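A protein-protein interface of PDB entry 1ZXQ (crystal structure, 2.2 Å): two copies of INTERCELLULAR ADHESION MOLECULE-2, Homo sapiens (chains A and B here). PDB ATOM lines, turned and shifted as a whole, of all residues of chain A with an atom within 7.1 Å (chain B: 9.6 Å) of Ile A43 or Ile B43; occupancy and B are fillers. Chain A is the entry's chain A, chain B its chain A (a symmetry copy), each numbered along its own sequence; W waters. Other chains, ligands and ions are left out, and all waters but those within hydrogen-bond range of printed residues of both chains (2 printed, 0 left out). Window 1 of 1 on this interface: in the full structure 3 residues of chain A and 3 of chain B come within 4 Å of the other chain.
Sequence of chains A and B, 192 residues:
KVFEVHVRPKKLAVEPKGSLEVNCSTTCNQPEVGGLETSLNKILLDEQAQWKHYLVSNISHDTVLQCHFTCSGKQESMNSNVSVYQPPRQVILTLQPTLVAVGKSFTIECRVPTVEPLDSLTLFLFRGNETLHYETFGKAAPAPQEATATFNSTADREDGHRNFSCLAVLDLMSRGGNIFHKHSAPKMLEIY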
ATOM      1  N   LEU A  40      -5.291  20.867 -10.082  1.00  0.00           N
ATOM      2  CA  LEU A  40      -3.852  20.702  -9.944  1.00  0.00           C
ATOM      3  C   LEU A  40      -3.359  21.338  -8.632  1.00  0.00           C
ATOM      4  O   LEU A  40      -4.117  22.043  -7.962  1.00  0.00           O
ATOM      5  CB  LEU A  40      -3.192  21.437 -11.085  1.00  0.00           C
ATOM      6  CG  LEU A  40      -3.596  20.992 -12.471  1.00  0.00           C
ATOM      7  CD1 LEU A  40      -3.178  22.041 -13.479  1.00  0.00           C
ATOM      8  CD2 LEU A  40      -2.960  19.668 -12.735  1.00  0.00           C
ATOM      9  N   ASN A  41      -2.095  21.116  -8.266  1.00  0.00           N
ATOM     10  CA  ASN A  41      -1.517  21.726  -7.063  1.00  0.00           C
ATOM     11  C   ASN A  41      -1.316  23.179  -7.412  1.00  0.00           C
ATOM     12  O   ASN A  41      -0.946  23.452  -8.544  1.00  0.00           O
ATOM     13  CB  ASN A  41      -0.145  21.143  -6.769  1.00  0.00           C
ATOM     14  CG  ASN A  41      -0.210  19.815  -6.042  1.00  0.00           C
ATOM     15  OD1 ASN A  41      -1.042  19.612  -5.126  1.00  0.00           O
ATOM     16  ND2 ASN A  41       0.681  18.908  -6.419  1.00  0.00           N
ATOM     17  N   LYS A  42      -1.548  24.107  -6.477  1.00  0.00           N
ATOM     18  CA  LYS A  42      -1.365  25.556  -6.715  1.00  0.00           C
ATOM     19  C   LYS A  42      -0.753  26.277  -5.497  1.00  0.00           C
ATOM     20  O   LYS A  42      -0.995  25.892  -4.349  1.00  0.00           O
ATOM     21  CB  LYS A  42      -2.681  26.215  -7.085  1.00  0.00           C
ATOM     22  CG  LYS A  42      -3.710  26.116  -6.013  1.00  0.00           C
ATOM     23  CD  LYS A  42      -4.960  26.871  -6.353  1.00  0.00           C
ATOM     24  CE  LYS A  42      -5.914  26.742  -5.199  1.00  0.00           C
ATOM     25  NZ  LYS A  42      -7.250  27.075  -5.660  1.00  0.00           N
ATOM     26  N   ILE A  43       0.055  27.301  -5.767  1.00  0.00           N
ATOM     27  CA  ILE A  43       0.735  28.083  -4.742  1.00  0.00           C
ATOM     28  C   ILE A  43       0.375  29.530  -4.981  1.00  0.00           C
ATOM     29  O   ILE A  43       0.633  30.053  -6.054  1.00  0.00           O
ATOM     30  CB  ILE A  43       2.272  28.008  -4.903  1.00  0.00           C
ATOM     31  CG1 ILE A  43       2.761  26.572  -4.817  1.00  0.00           C
ATOM     32  CG2 ILE A  43       2.956  28.793  -3.806  1.00  0.00           C
ATOM     33  CD1 ILE A  43       2.455  25.902  -3.483  1.00  0.00           C
ATOM     34  N   LEU A  44      -0.248  30.191  -4.021  1.00  0.00           N
ATOM     35  CA  LEU A  44      -0.525  31.586  -4.246  1.00  0.00           C
ATOM     36  C   LEU A  44       0.819  32.240  -4.051  1.00  0.00           C
ATOM     37  O   LEU A  44       1.426  32.167  -2.979  1.00  0.00           O
ATOM     38  CB  LEU A  44      -1.498  32.145  -3.239  1.00  0.00           C
ATOM     39  CG  LEU A  44      -1.697  33.642  -3.391  1.00  0.00           C
ATOM     40  CD1 LEU A  44      -2.419  34.002  -4.644  1.00  0.00           C
ATOM     41  CD2 LEU A  44      -2.484  34.059  -2.235  1.00  0.00           C
ATOM     42  N   LEU A  45       1.327  32.787  -5.132  1.00  0.00           N
ATOM     43  CA  LEU A  45       2.594  33.445  -5.079  1.00  0.00           C
ATOM     44  C   LEU A  45       2.442  34.866  -4.541  1.00  0.00           C
ATOM     45  O   LEU A  45       3.278  35.339  -3.762  1.00  0.00           O
ATOM     46  CB  LEU A  45       3.228  33.487  -6.455  1.00  0.00           C
ATOM     47  CG  LEU A  45       3.485  32.162  -7.132  1.00  0.00           C
ATOM     48  CD1 LEU A  45       4.051  32.500  -8.512  1.00  0.00           C
ATOM     49  CD2 LEU A  45       4.407  31.279  -6.283  1.00  0.00           C
ATOM     50  N   ASP A  46       1.409  35.575  -4.964  1.00  0.00           N
ATOM     51  CA  ASP A  46       1.255  36.926  -4.479  1.00  0.00           C
ATOM     52  C   ASP A  46      -0.117  37.460  -4.827  1.00  0.00           C
ATOM     53  O   ASP A  46      -0.725  37.008  -5.790  1.00  0.00           O
ATOM     54  CB  ASP A  46       2.338  37.803  -5.094  1.00  0.00           C
ATOM     55  CG  ASP A  46       2.658  39.035  -4.237  1.00  0.00           C
ATOM     56  OD1 ASP A  46       2.449  39.023  -2.985  1.00  0.00           O
ATOM     57  OD2 ASP A  46       3.133  40.030  -4.829  1.00  0.00           O
ATOM     58  N   HIS A  53      -2.001  35.963  -7.966  1.00  0.00           N
ATOM     59  CA  HIS A  53      -1.068  35.390  -8.891  1.00  0.00           C
ATOM     60  C   HIS A  53      -0.705  34.043  -8.284  1.00  0.00           C
ATOM     61  O   HIS A  53      -0.257  33.998  -7.138  1.00  0.00           O
ATOM     62  CB  HIS A  53       0.133  36.342  -8.911  1.00  0.00           C
ATOM     63  CG  HIS A  53       1.204  35.956  -9.876  1.00  0.00           C
ATOM     64  ND1 HIS A  53       1.031  36.017 -11.247  1.00  0.00           N
ATOM     65  CD2 HIS A  53       2.450  35.466  -9.676  1.00  0.00           C
ATOM     66  CE1 HIS A  53       2.126  35.578 -11.846  1.00  0.00           C
ATOM     67  NE2 HIS A  53       2.999  35.235 -10.916  1.00  0.00           N
ATOM     68  N   TYR A  54      -0.931  32.952  -9.015  1.00  0.00           N
ATOM     69  CA  TYR A  54      -0.647  31.613  -8.509  1.00  0.00           C
ATOM     70  C   TYR A  54       0.276  30.958  -9.466  1.00  0.00           C
ATOM     71  O   TYR A  54       0.357  31.372 -10.597  1.00  0.00           O
ATOM     72  CB  TYR A  54      -1.907  30.716  -8.538  1.00  0.00           C
ATOM     73  CG  TYR A  54      -3.102  31.086  -7.672  1.00  0.00           C
ATOM     74  CD1 TYR A  54      -3.918  32.171  -8.004  1.00  0.00           C
ATOM     75  CD2 TYR A  54      -3.433  30.333  -6.545  1.00  0.00           C
ATOM     76  CE1 TYR A  54      -5.024  32.493  -7.245  1.00  0.00           C
ATOM     77  CE2 TYR A  54      -4.523  30.656  -5.788  1.00  0.00           C
ATOM     78  CZ  TYR A  54      -5.313  31.740  -6.146  1.00  0.00           C
ATOM     79  OH  TYR A  54      -6.389  32.113  -5.400  1.00  0.00           O
ATOM     80  N   LEU A  55       0.943  29.907  -9.017  1.00  0.00           N
ATOM     81  CA  LEU A  55       1.789  29.084  -9.901  1.00  0.00           C
ATOM     82  C   LEU A  55       1.044  27.756  -9.834  1.00  0.00           C
ATOM     83  O   LEU A  55       0.871  27.233  -8.723  1.00  0.00           O
ATOM     84  CB  LEU A  55       3.211  28.836  -9.361  1.00  0.00           C
ATOM     85  CG  LEU A  55       4.008  27.666  -9.998  1.00  0.00           C
ATOM     86  CD1 LEU A  55       4.424  28.043 -11.376  1.00  0.00           C
ATOM     87  CD2 LEU A  55       5.237  27.287  -9.177  1.00  0.00           C
ATOM     88  N   VAL A  56       0.523  27.273 -10.969  1.00  0.00           N
ATOM     89  CA  VAL A  56      -0.211  26.007 -11.029  1.00  0.00           C
ATOM     90  C   VAL A  56       0.793  25.004 -11.591  1.00  0.00           C
ATOM     91  O   VAL A  56       1.531  25.350 -12.504  1.00  0.00           O
ATOM     92  CB  VAL A  56      -1.439  26.148 -11.930  1.00  0.00           C
ATOM     93  CG1 VAL A  56      -2.249  24.900 -11.908  1.00  0.00           C
ATOM     94  CG2 VAL A  56      -2.302  27.264 -11.429  1.00  0.00           C
ATOM     95  N   SER A  57       0.854  23.781 -11.056  1.00  0.00           N
ATOM     96  CA  SER A  57       1.863  22.844 -11.553  1.00  0.00           C
ATOM     97  C   SER A  57       1.574  21.345 -11.774  1.00  0.00           C
ATOM     98  O   SER A  57       0.569  20.800 -11.309  1.00  0.00           O
ATOM     99  CB  SER A  57       3.141  23.003 -10.716  1.00  0.00           C
ATOM    100  OG  SER A  57       2.907  22.725  -9.356  1.00  0.00           O
ATOM    101  N   SER B  19       7.663  24.524   7.909  1.00  0.00           N
ATOM    102  CA  SER B  19       6.716  23.757   7.183  1.00  0.00           C
ATOM    103  C   SER B  19       6.536  22.421   7.843  1.00  0.00           C
ATOM    104  O   SER B  19       7.204  22.109   8.822  1.00  0.00           O
ATOM    105  CB  SER B  19       7.205  23.640   5.737  1.00  0.00           C
ATOM    106  OG  SER B  19       8.207  22.646   5.554  1.00  0.00           O
ATOM    107  N   LEU B  20       5.575  21.659   7.348  1.00  0.00           N
ATOM    108  CA  LEU B  20       5.302  20.329   7.880  1.00  0.00           C
ATOM    109  C   LEU B  20       4.444  19.408   6.984  1.00  0.00           C
ATOM    110  O   LEU B  20       3.721  19.872   6.093  1.00  0.00           O
ATOM    111  CB  LEU B  20       4.678  20.419   9.273  1.00  0.00           C
ATOM    112  CG  LEU B  20       3.199  20.696   9.333  1.00  0.00           C
ATOM    113  CD1 LEU B  20       2.573  19.870  10.409  1.00  0.00           C
ATOM    114  CD2 LEU B  20       3.013  22.136   9.546  1.00  0.00           C
ATOM    115  N   GLU B  21       4.573  18.101   7.205  1.00  0.00           N
ATOM    116  CA  GLU B  21       3.822  17.114   6.466  1.00  0.00           C
ATOM    117  C   GLU B  21       2.705  16.620   7.354  1.00  0.00           C
ATOM    118  O   GLU B  21       2.904  16.400   8.547  1.00  0.00           O
ATOM    119  CB  GLU B  21       4.738  15.975   6.066  1.00  0.00           C
ATOM    120  CG  GLU B  21       5.842  16.446   5.174  1.00  0.00           C
ATOM    121  CD  GLU B  21       6.608  15.305   4.496  1.00  0.00           C
ATOM    122  OE1 GLU B  21       6.601  14.132   4.992  1.00  0.00           O
ATOM    123  OE2 GLU B  21       7.240  15.592   3.448  1.00  0.00           O
ATOM    124  N   VAL B  22       1.522  16.487   6.768  1.00  0.00           N
ATOM    125  CA  VAL B  22       0.342  16.057   7.483  1.00  0.00           C
ATOM    126  C   VAL B  22      -0.232  14.880   6.750  1.00  0.00           C
ATOM    127  O   VAL B  22      -0.294  14.869   5.528  1.00  0.00           O
ATOM    128  CB  VAL B  22      -0.728  17.119   7.451  1.00  0.00           C
ATOM    129  CG1 VAL B  22      -1.801  16.768   8.433  1.00  0.00           C
ATOM    130  CG2 VAL B  22      -0.139  18.478   7.734  1.00  0.00           C
ATOM    131  N   ASN B  23      -0.576  13.845   7.493  1.00  0.00           N
ATOM    132  CA  ASN B  23      -1.163  12.660   6.919  1.00  0.00           C
ATOM    133  C   ASN B  23      -2.557  12.602   7.484  1.00  0.00           C
ATOM    134  O   ASN B  23      -2.776  12.339   8.657  1.00  0.00           O
ATOM    135  CB  ASN B  23      -0.374  11.388   7.244  1.00  0.00           C
ATOM    136  CG  ASN B  23      -0.890  10.178   6.455  1.00  0.00           C
ATOM    137  OD1 ASN B  23      -1.994  10.189   5.914  1.00  0.00           O
ATOM    138  ND2 ASN B  23      -0.082   9.139   6.346  1.00  0.00           N
ATOM    139  N   LEU B  36      -7.642  18.281   3.410  1.00  0.00           N
ATOM    140  CA  LEU B  36      -7.054  18.982   4.540  1.00  0.00           C
ATOM    141  C   LEU B  36      -7.295  20.437   4.219  1.00  0.00           C
ATOM    142  O   LEU B  36      -6.873  20.912   3.175  1.00  0.00           O
ATOM    143  CB  LEU B  36      -5.553  18.742   4.604  1.00  0.00           C
ATOM    144  CG  LEU B  36      -4.793  19.320   5.792  1.00  0.00           C
ATOM    145  CD1 LEU B  36      -5.185  18.600   7.064  1.00  0.00           C
ATOM    146  CD2 LEU B  36      -3.318  19.152   5.539  1.00  0.00           C
ATOM    147  N   THR B  38      -6.793  24.421   5.045  1.00  0.00           N
ATOM    148  CA  THR B  38      -5.839  25.257   5.736  1.00  0.00           C
ATOM    149  C   THR B  38      -5.720  26.601   5.053  1.00  0.00           C
ATOM    150  O   THR B  38      -6.076  26.737   3.902  1.00  0.00           O
ATOM    151  CB  THR B  38      -4.453  24.572   5.799  1.00  0.00           C
ATOM    152  OG1 THR B  38      -3.493  25.515   6.294  1.00  0.00           O
ATOM    153  CG2 THR B  38      -4.021  24.039   4.431  1.00  0.00           C
ATOM    154  N   LEU B  40      -2.860  28.095   4.815  1.00  0.00           N
ATOM    155  CA  LEU B  40      -1.504  28.121   4.288  1.00  0.00           C
ATOM    156  C   LEU B  40      -1.451  27.457   2.900  1.00  0.00           C
ATOM    157  O   LEU B  40      -2.428  26.839   2.472  1.00  0.00           O
ATOM    158  CB  LEU B  40      -0.633  27.309   5.217  1.00  0.00           C
ATOM    159  CG  LEU B  40      -0.600  27.773   6.655  1.00  0.00           C
ATOM    160  CD1 LEU B  40      -0.028  26.674   7.524  1.00  0.00           C
ATOM    161  CD2 LEU B  40       0.210  29.025   6.717  1.00  0.00           C
ATOM    162  N   ASN B  41      -0.319  27.561   2.201  1.00  0.00           N
ATOM    163  CA  ASN B  41      -0.153  26.913   0.895  1.00  0.00           C
ATOM    164  C   ASN B  41      -0.006  25.443   1.196  1.00  0.00           C
ATOM    165  O   ASN B  41       0.629  25.119   2.188  1.00  0.00           O
ATOM    166  CB  ASN B  41       1.138  27.364   0.231  1.00  0.00           C
ATOM    167  CG  ASN B  41       1.007  28.701  -0.469  1.00  0.00           C
ATOM    168  OD1 ASN B  41      -0.019  28.997  -1.127  1.00  0.00           O
ATOM    169  ND2 ASN B  41       2.051  29.512  -0.361  1.00  0.00           N
ATOM    170  N   LYS B  42      -0.573  24.555   0.372  1.00  0.00           N
ATOM    171  CA  LYS B  42      -0.475  23.092   0.571  1.00  0.00           C
ATOM    172  C   LYS B  42      -0.291  22.331  -0.758  1.00  0.00           C
ATOM    173  O   LYS B  42      -0.798  22.753  -1.802  1.00  0.00           O
ATOM    174  CB  LYS B  42      -1.699  22.559   1.293  1.00  0.00           C
ATOM    175  CG  LYS B  42      -2.966  22.772   0.541  1.00  0.00           C
ATOM    176  CD  LYS B  42      -4.143  22.138   1.218  1.00  0.00           C
ATOM    177  CE  LYS B  42      -5.358  22.375   0.365  1.00  0.00           C
ATOM    178  NZ  LYS B  42      -6.544  22.168   1.177  1.00  0.00           N
ATOM    179  N   ILE B  43       0.456  21.230  -0.704  1.00  0.00           N
ATOM    180  CA  ILE B  43       0.752  20.399  -1.865  1.00  0.00           C
ATOM    181  C   ILE B  43       0.331  18.990  -1.518  1.00  0.00           C
ATOM    182  O   ILE B  43       0.819  18.431  -0.548  1.00  0.00           O
ATOM    183  CB  ILE B  43       2.275  20.322  -2.129  1.00  0.00           C
ATOM    184  CG1 ILE B  43       2.860  21.704  -2.365  1.00  0.00           C
ATOM    185  CG2 ILE B  43       2.554  19.488  -3.360  1.00  0.00           C
ATOM    186  CD1 ILE B  43       2.269  22.418  -3.574  1.00  0.00           C
ATOM    187  N   LEU B  44      -0.591  18.407  -2.262  1.00  0.00           N
ATOM    188  CA  LEU B  44      -0.931  17.042  -1.952  1.00  0.00           C
ATOM    189  C   LEU B  44       0.239  16.263  -2.496  1.00  0.00           C
ATOM    190  O   LEU B  44       0.535  16.292  -3.694  1.00  0.00           O
ATOM    191  CB  LEU B  44      -2.190  16.595  -2.648  1.00  0.00           C
ATOM    192  CG  LEU B  44      -2.486  15.122  -2.427  1.00  0.00           C
ATOM    193  CD1 LEU B  44      -2.872  14.817  -1.021  1.00  0.00           C
ATOM    194  CD2 LEU B  44      -3.594  14.800  -3.320  1.00  0.00           C
ATOM    195  N   LEU B  45       0.966  15.655  -1.586  1.00  0.00           N
ATOM    196  CA  LEU B  45       2.101  14.877  -1.974  1.00  0.00           C
ATOM    197  C   LEU B  45       1.670  13.485  -2.430  1.00  0.00           C
ATOM    198  O   LEU B  45       2.212  12.944  -3.401  1.00  0.00           O
ATOM    199  CB  LEU B  45       3.078  14.755  -0.821  1.00  0.00           C
ATOM    200  CG  LEU B  45       3.637  16.039  -0.259  1.00  0.00           C
ATOM    201  CD1 LEU B  45       4.522  15.629   0.920  1.00  0.00           C
ATOM    202  CD2 LEU B  45       4.375  16.839  -1.338  1.00  0.00           C
ATOM    203  N   ASP B  46       0.727  12.874  -1.733  1.00  0.00           N
ATOM    204  CA  ASP B  46       0.316  11.551  -2.139  1.00  0.00           C
ATOM    205  C   ASP B  46      -0.955  11.149  -1.424  1.00  0.00           C
ATOM    206  O   ASP B  46      -1.232  11.645  -0.338  1.00  0.00           O
ATOM    207  CB  ASP B  46       1.435  10.564  -1.831  1.00  0.00           C
ATOM    208  CG  ASP B  46       1.388   9.319  -2.725  1.00  0.00           C
ATOM    209  OD1 ASP B  46       0.847   9.368  -3.873  1.00  0.00           O
ATOM    210  OD2 ASP B  46       1.906   8.275  -2.271  1.00  0.00           O
ATOM    211  N   GLU B  47      -1.747  10.282  -2.053  1.00  0.00           N
ATOM    212  CA  GLU B  47      -3.015   9.802  -1.477  1.00  0.00           C
ATOM    213  C   GLU B  47      -3.311   8.378  -1.875  1.00  0.00           C
ATOM    214  O   GLU B  47      -2.675   7.825  -2.771  1.00  0.00           O
ATOM    215  CB  GLU B  47      -4.212  10.641  -1.950  1.00  0.00           C
ATOM    216  CG  GLU B  47      -4.503  10.527  -3.412  1.00  0.00           C
ATOM    217  CD  GLU B  47      -5.571  11.478  -3.833  1.00  0.00           C
ATOM    218  OE1 GLU B  47      -6.579  11.553  -3.100  1.00  0.00           O
ATOM    219  OE2 GLU B  47      -5.405  12.178  -4.864  1.00  0.00           O
ATOM    220  N   LYS B  52      -4.558  10.940   2.701  1.00  0.00           N
ATOM    221  CA  LYS B  52      -3.981  11.989   1.878  1.00  0.00           C
ATOM    222  C   LYS B  52      -2.886  12.563   2.718  1.00  0.00           C
ATOM    223  O   LYS B  52      -3.035  12.734   3.900  1.00  0.00           O
ATOM    224  CB  LYS B  52      -5.004  13.032   1.529  1.00  0.00           C
ATOM    225  CG  LYS B  52      -6.073  12.468   0.653  1.00  0.00           C
ATOM    226  CD  LYS B  52      -7.155  13.471   0.387  1.00  0.00           C
ATOM    227  CE  LYS B  52      -6.722  14.448  -0.652  1.00  0.00           C
ATOM    228  NZ  LYS B  52      -7.874  15.225  -1.115  1.00  0.00           N
ATOM    229  N   HIS B  53      -1.759  12.780   2.088  1.00  0.00           N
ATOM    230  CA  HIS B  53      -0.558  13.247   2.717  1.00  0.00           C
ATOM    231  C   HIS B  53      -0.245  14.560   2.016  1.00  0.00           C
ATOM    232  O   HIS B  53      -0.123  14.577   0.791  1.00  0.00           O
ATOM    233  CB  HIS B  53       0.504  12.182   2.423  1.00  0.00           C
ATOM    234  CG  HIS B  53       1.829  12.448   3.054  1.00  0.00           C
ATOM    235  ND1 HIS B  53       2.031  12.386   4.421  1.00  0.00           N
ATOM    236  CD2 HIS B  53       3.016  12.817   2.516  1.00  0.00           C
ATOM    237  CE1 HIS B  53       3.285  12.708   4.694  1.00  0.00           C
ATOM    238  NE2 HIS B  53       3.902  12.976   3.556  1.00  0.00           N
ATOM    239  N   TYR B  54      -0.155  15.658   2.766  1.00  0.00           N
ATOM    240  CA  TYR B  54       0.109  16.969   2.184  1.00  0.00           C
ATOM    241  C   TYR B  54       1.317  17.518   2.845  1.00  0.00           C
ATOM    242  O   TYR B  54       1.663  17.083   3.916  1.00  0.00           O
ATOM    243  CB  TYR B  54      -1.002  17.984   2.542  1.00  0.00           C
ATOM    244  CG  TYR B  54      -2.417  17.745   2.039  1.00  0.00           C
ATOM    245  CD1 TYR B  54      -3.213  16.740   2.595  1.00  0.00           C
ATOM    246  CD2 TYR B  54      -2.967  18.542   1.035  1.00  0.00           C
ATOM    247  CE1 TYR B  54      -4.511  16.538   2.170  1.00  0.00           C
ATOM    248  CE2 TYR B  54      -4.248  18.337   0.607  1.00  0.00           C
ATOM    249  CZ  TYR B  54      -5.013  17.330   1.181  1.00  0.00           C
ATOM    250  OH  TYR B  54      -6.282  17.074   0.761  1.00  0.00           O
ATOM    251  N   LEU B  55       1.936  18.505   2.217  1.00  0.00           N
ATOM    252  CA  LEU B  55       3.067  19.230   2.826  1.00  0.00           C
ATOM    253  C   LEU B  55       2.465  20.625   2.946  1.00  0.00           C
ATOM    254  O   LEU B  55       2.048  21.177   1.917  1.00  0.00           O
ATOM    255  CB  LEU B  55       4.305  19.345   1.916  1.00  0.00           C
ATOM    256  CG  LEU B  55       5.356  20.423   2.296  1.00  0.00           C
ATOM    257  CD1 LEU B  55       6.092  19.989   3.514  1.00  0.00           C
ATOM    258  CD2 LEU B  55       6.346  20.691   1.167  1.00  0.00           C
ATOM    259  N   VAL B  56       2.322  21.141   4.174  1.00  0.00           N
ATOM    260  CA  VAL B  56       1.760  22.471   4.413  1.00  0.00           C
ATOM    261  C   VAL B  56       2.971  23.364   4.668  1.00  0.00           C
ATOM    262  O   VAL B  56       3.892  22.935   5.351  1.00  0.00           O
ATOM    263  CB  VAL B  56       0.815  22.439   5.617  1.00  0.00           C
ATOM    264  CG1 VAL B  56       0.155  23.760   5.799  1.00  0.00           C
ATOM    265  CG2 VAL B  56      -0.256  21.419   5.385  1.00  0.00           C
ATOM    266  N   SER B  57       3.004  24.582   4.119  1.00  0.00           N
ATOM    267  CA  SER B  57       4.196  25.410   4.311  1.00  0.00           C
ATOM    268  C   SER B  57       4.126  26.927   4.582  1.00  0.00           C
ATOM    269  O   SER B  57       3.090  27.574   4.401  1.00  0.00           O
ATOM    270  CB  SER B  57       5.176  25.138   3.160  1.00  0.00           C
ATOM    271  OG  SER B  57       4.609  25.457   1.911  1.00  0.00           O
ATOM    272  N   ASN B  58       5.258  27.477   5.017  1.00  0.00           N
ATOM    273  CA  ASN B  58       5.371  28.883   5.303  1.00  0.00           C
ATOM    274  C   ASN B  58       4.396  29.319   6.385  1.00  0.00           C
ATOM    275  O   ASN B  58       3.525  30.160   6.190  1.00  0.00           O
ATOM    276  CB  ASN B  58       5.187  29.678   4.037  1.00  0.00           C
ATOM    277  CG  ASN B  58       5.756  31.047   4.150  1.00  0.00           C
ATOM    278  OD1 ASN B  58       6.873  31.239   4.632  1.00  0.00           O
ATOM    279  ND2 ASN B  58       4.984  32.014   3.680  1.00  0.00           N
HETATM  280  O   HOH W   1      -2.001  26.178  -1.811  1.00  0.00           O
HETATM  281  O   HOH W   2      -2.479  22.601  -3.967  1.00  0.00           O
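OD1 of Asn A41 is in hydrogen-bond range of N of Leu B44 (3.1 Å). N of Leu A44 sits at hydrogen-bond distance from OD1 of Asn B41 (3.1 Å).
The backbone carbonyl oxygen of Asn A41 lies within hydrogen-bond range of the backbone NH of Ser A57 (3.1 Å). O of Ile A43 lies within hydrogen-bond range of N of Leu A55, at 3.0 Å. N of Ser B57 lies within hydrogen-bond range of O of Asn B41. N of Leu B55 sits at hydrogen-bond distance from O of Ile B43, 3.0 Å away.
Among the printed residues, pairs that only touch across the chains: Asn A41 with Ile B43, Ile A43 with Asn B41 and Ile A43 with Ile B43.
Printed residues of chain B within 4 Å of Asn A41: Ile B43 (3.6 Å) and Leu B44 (3.1 Å). Printed residues of chain B within 4 Å of Leu A44: Asn B41. Leu B20 touches none of the printed residues of chain A. Printed residues of chain A within 4 Å of Asn B41: Ile A43 (3.6 Å) and Leu A44 (3.1 Å). Of chain A, only Asn A41 (3.6 Å) and Ile A43 (3.5 Å) come within 4 Å of Ile B43. Printed residues of chain A within 4 Å of Leu B44: Asn A41 (3.1 Å). The nearest residue of chain A that does not touch Ile B43 is Lys A42 (4.8 Å). The nearest printed residue of chain B that does not touch Leu A44 is Lys B42 (7.2 Å).
Hydrophobic or aromatic side chains of chain A within 4 Å of the printed part of chain B: Ile A43. Of the 22 printed residues of chain B, 3 touch a printed residue of chain A. Printed residues of chain B that touch a printed residue of chain A: Asn B41, Ile B43 and Leu B44. Among the printed residues, 5 pairs touch across the chains. Among the printed residues, no Asp or Glu carboxylate lies within 4 Å of a Lys or Arg side-chain nitrogen of the other chain.
Asn A41 touches Ile B43, and with the chains exchanged Ile A43 touches Asn B41. Asn A41 touches Leu B44, and with the chains exchanged Leu A44 touches Asn B41. Ile A43 touches its own counterpart, Ile B43. Positions printed for both chains: 40, 41, 42, 43, 44, 45, 46, 53, 54, 55, 56 and 57.
Water W1 lies within hydrogen-bond range of O of Lys A42 (2.7 Å) and N of Lys B42 (3.1 Å). Water W2 bridges the backbone carbonyl oxygen (O) of Lys B42 and the backbone NH (N) of Lys A42.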
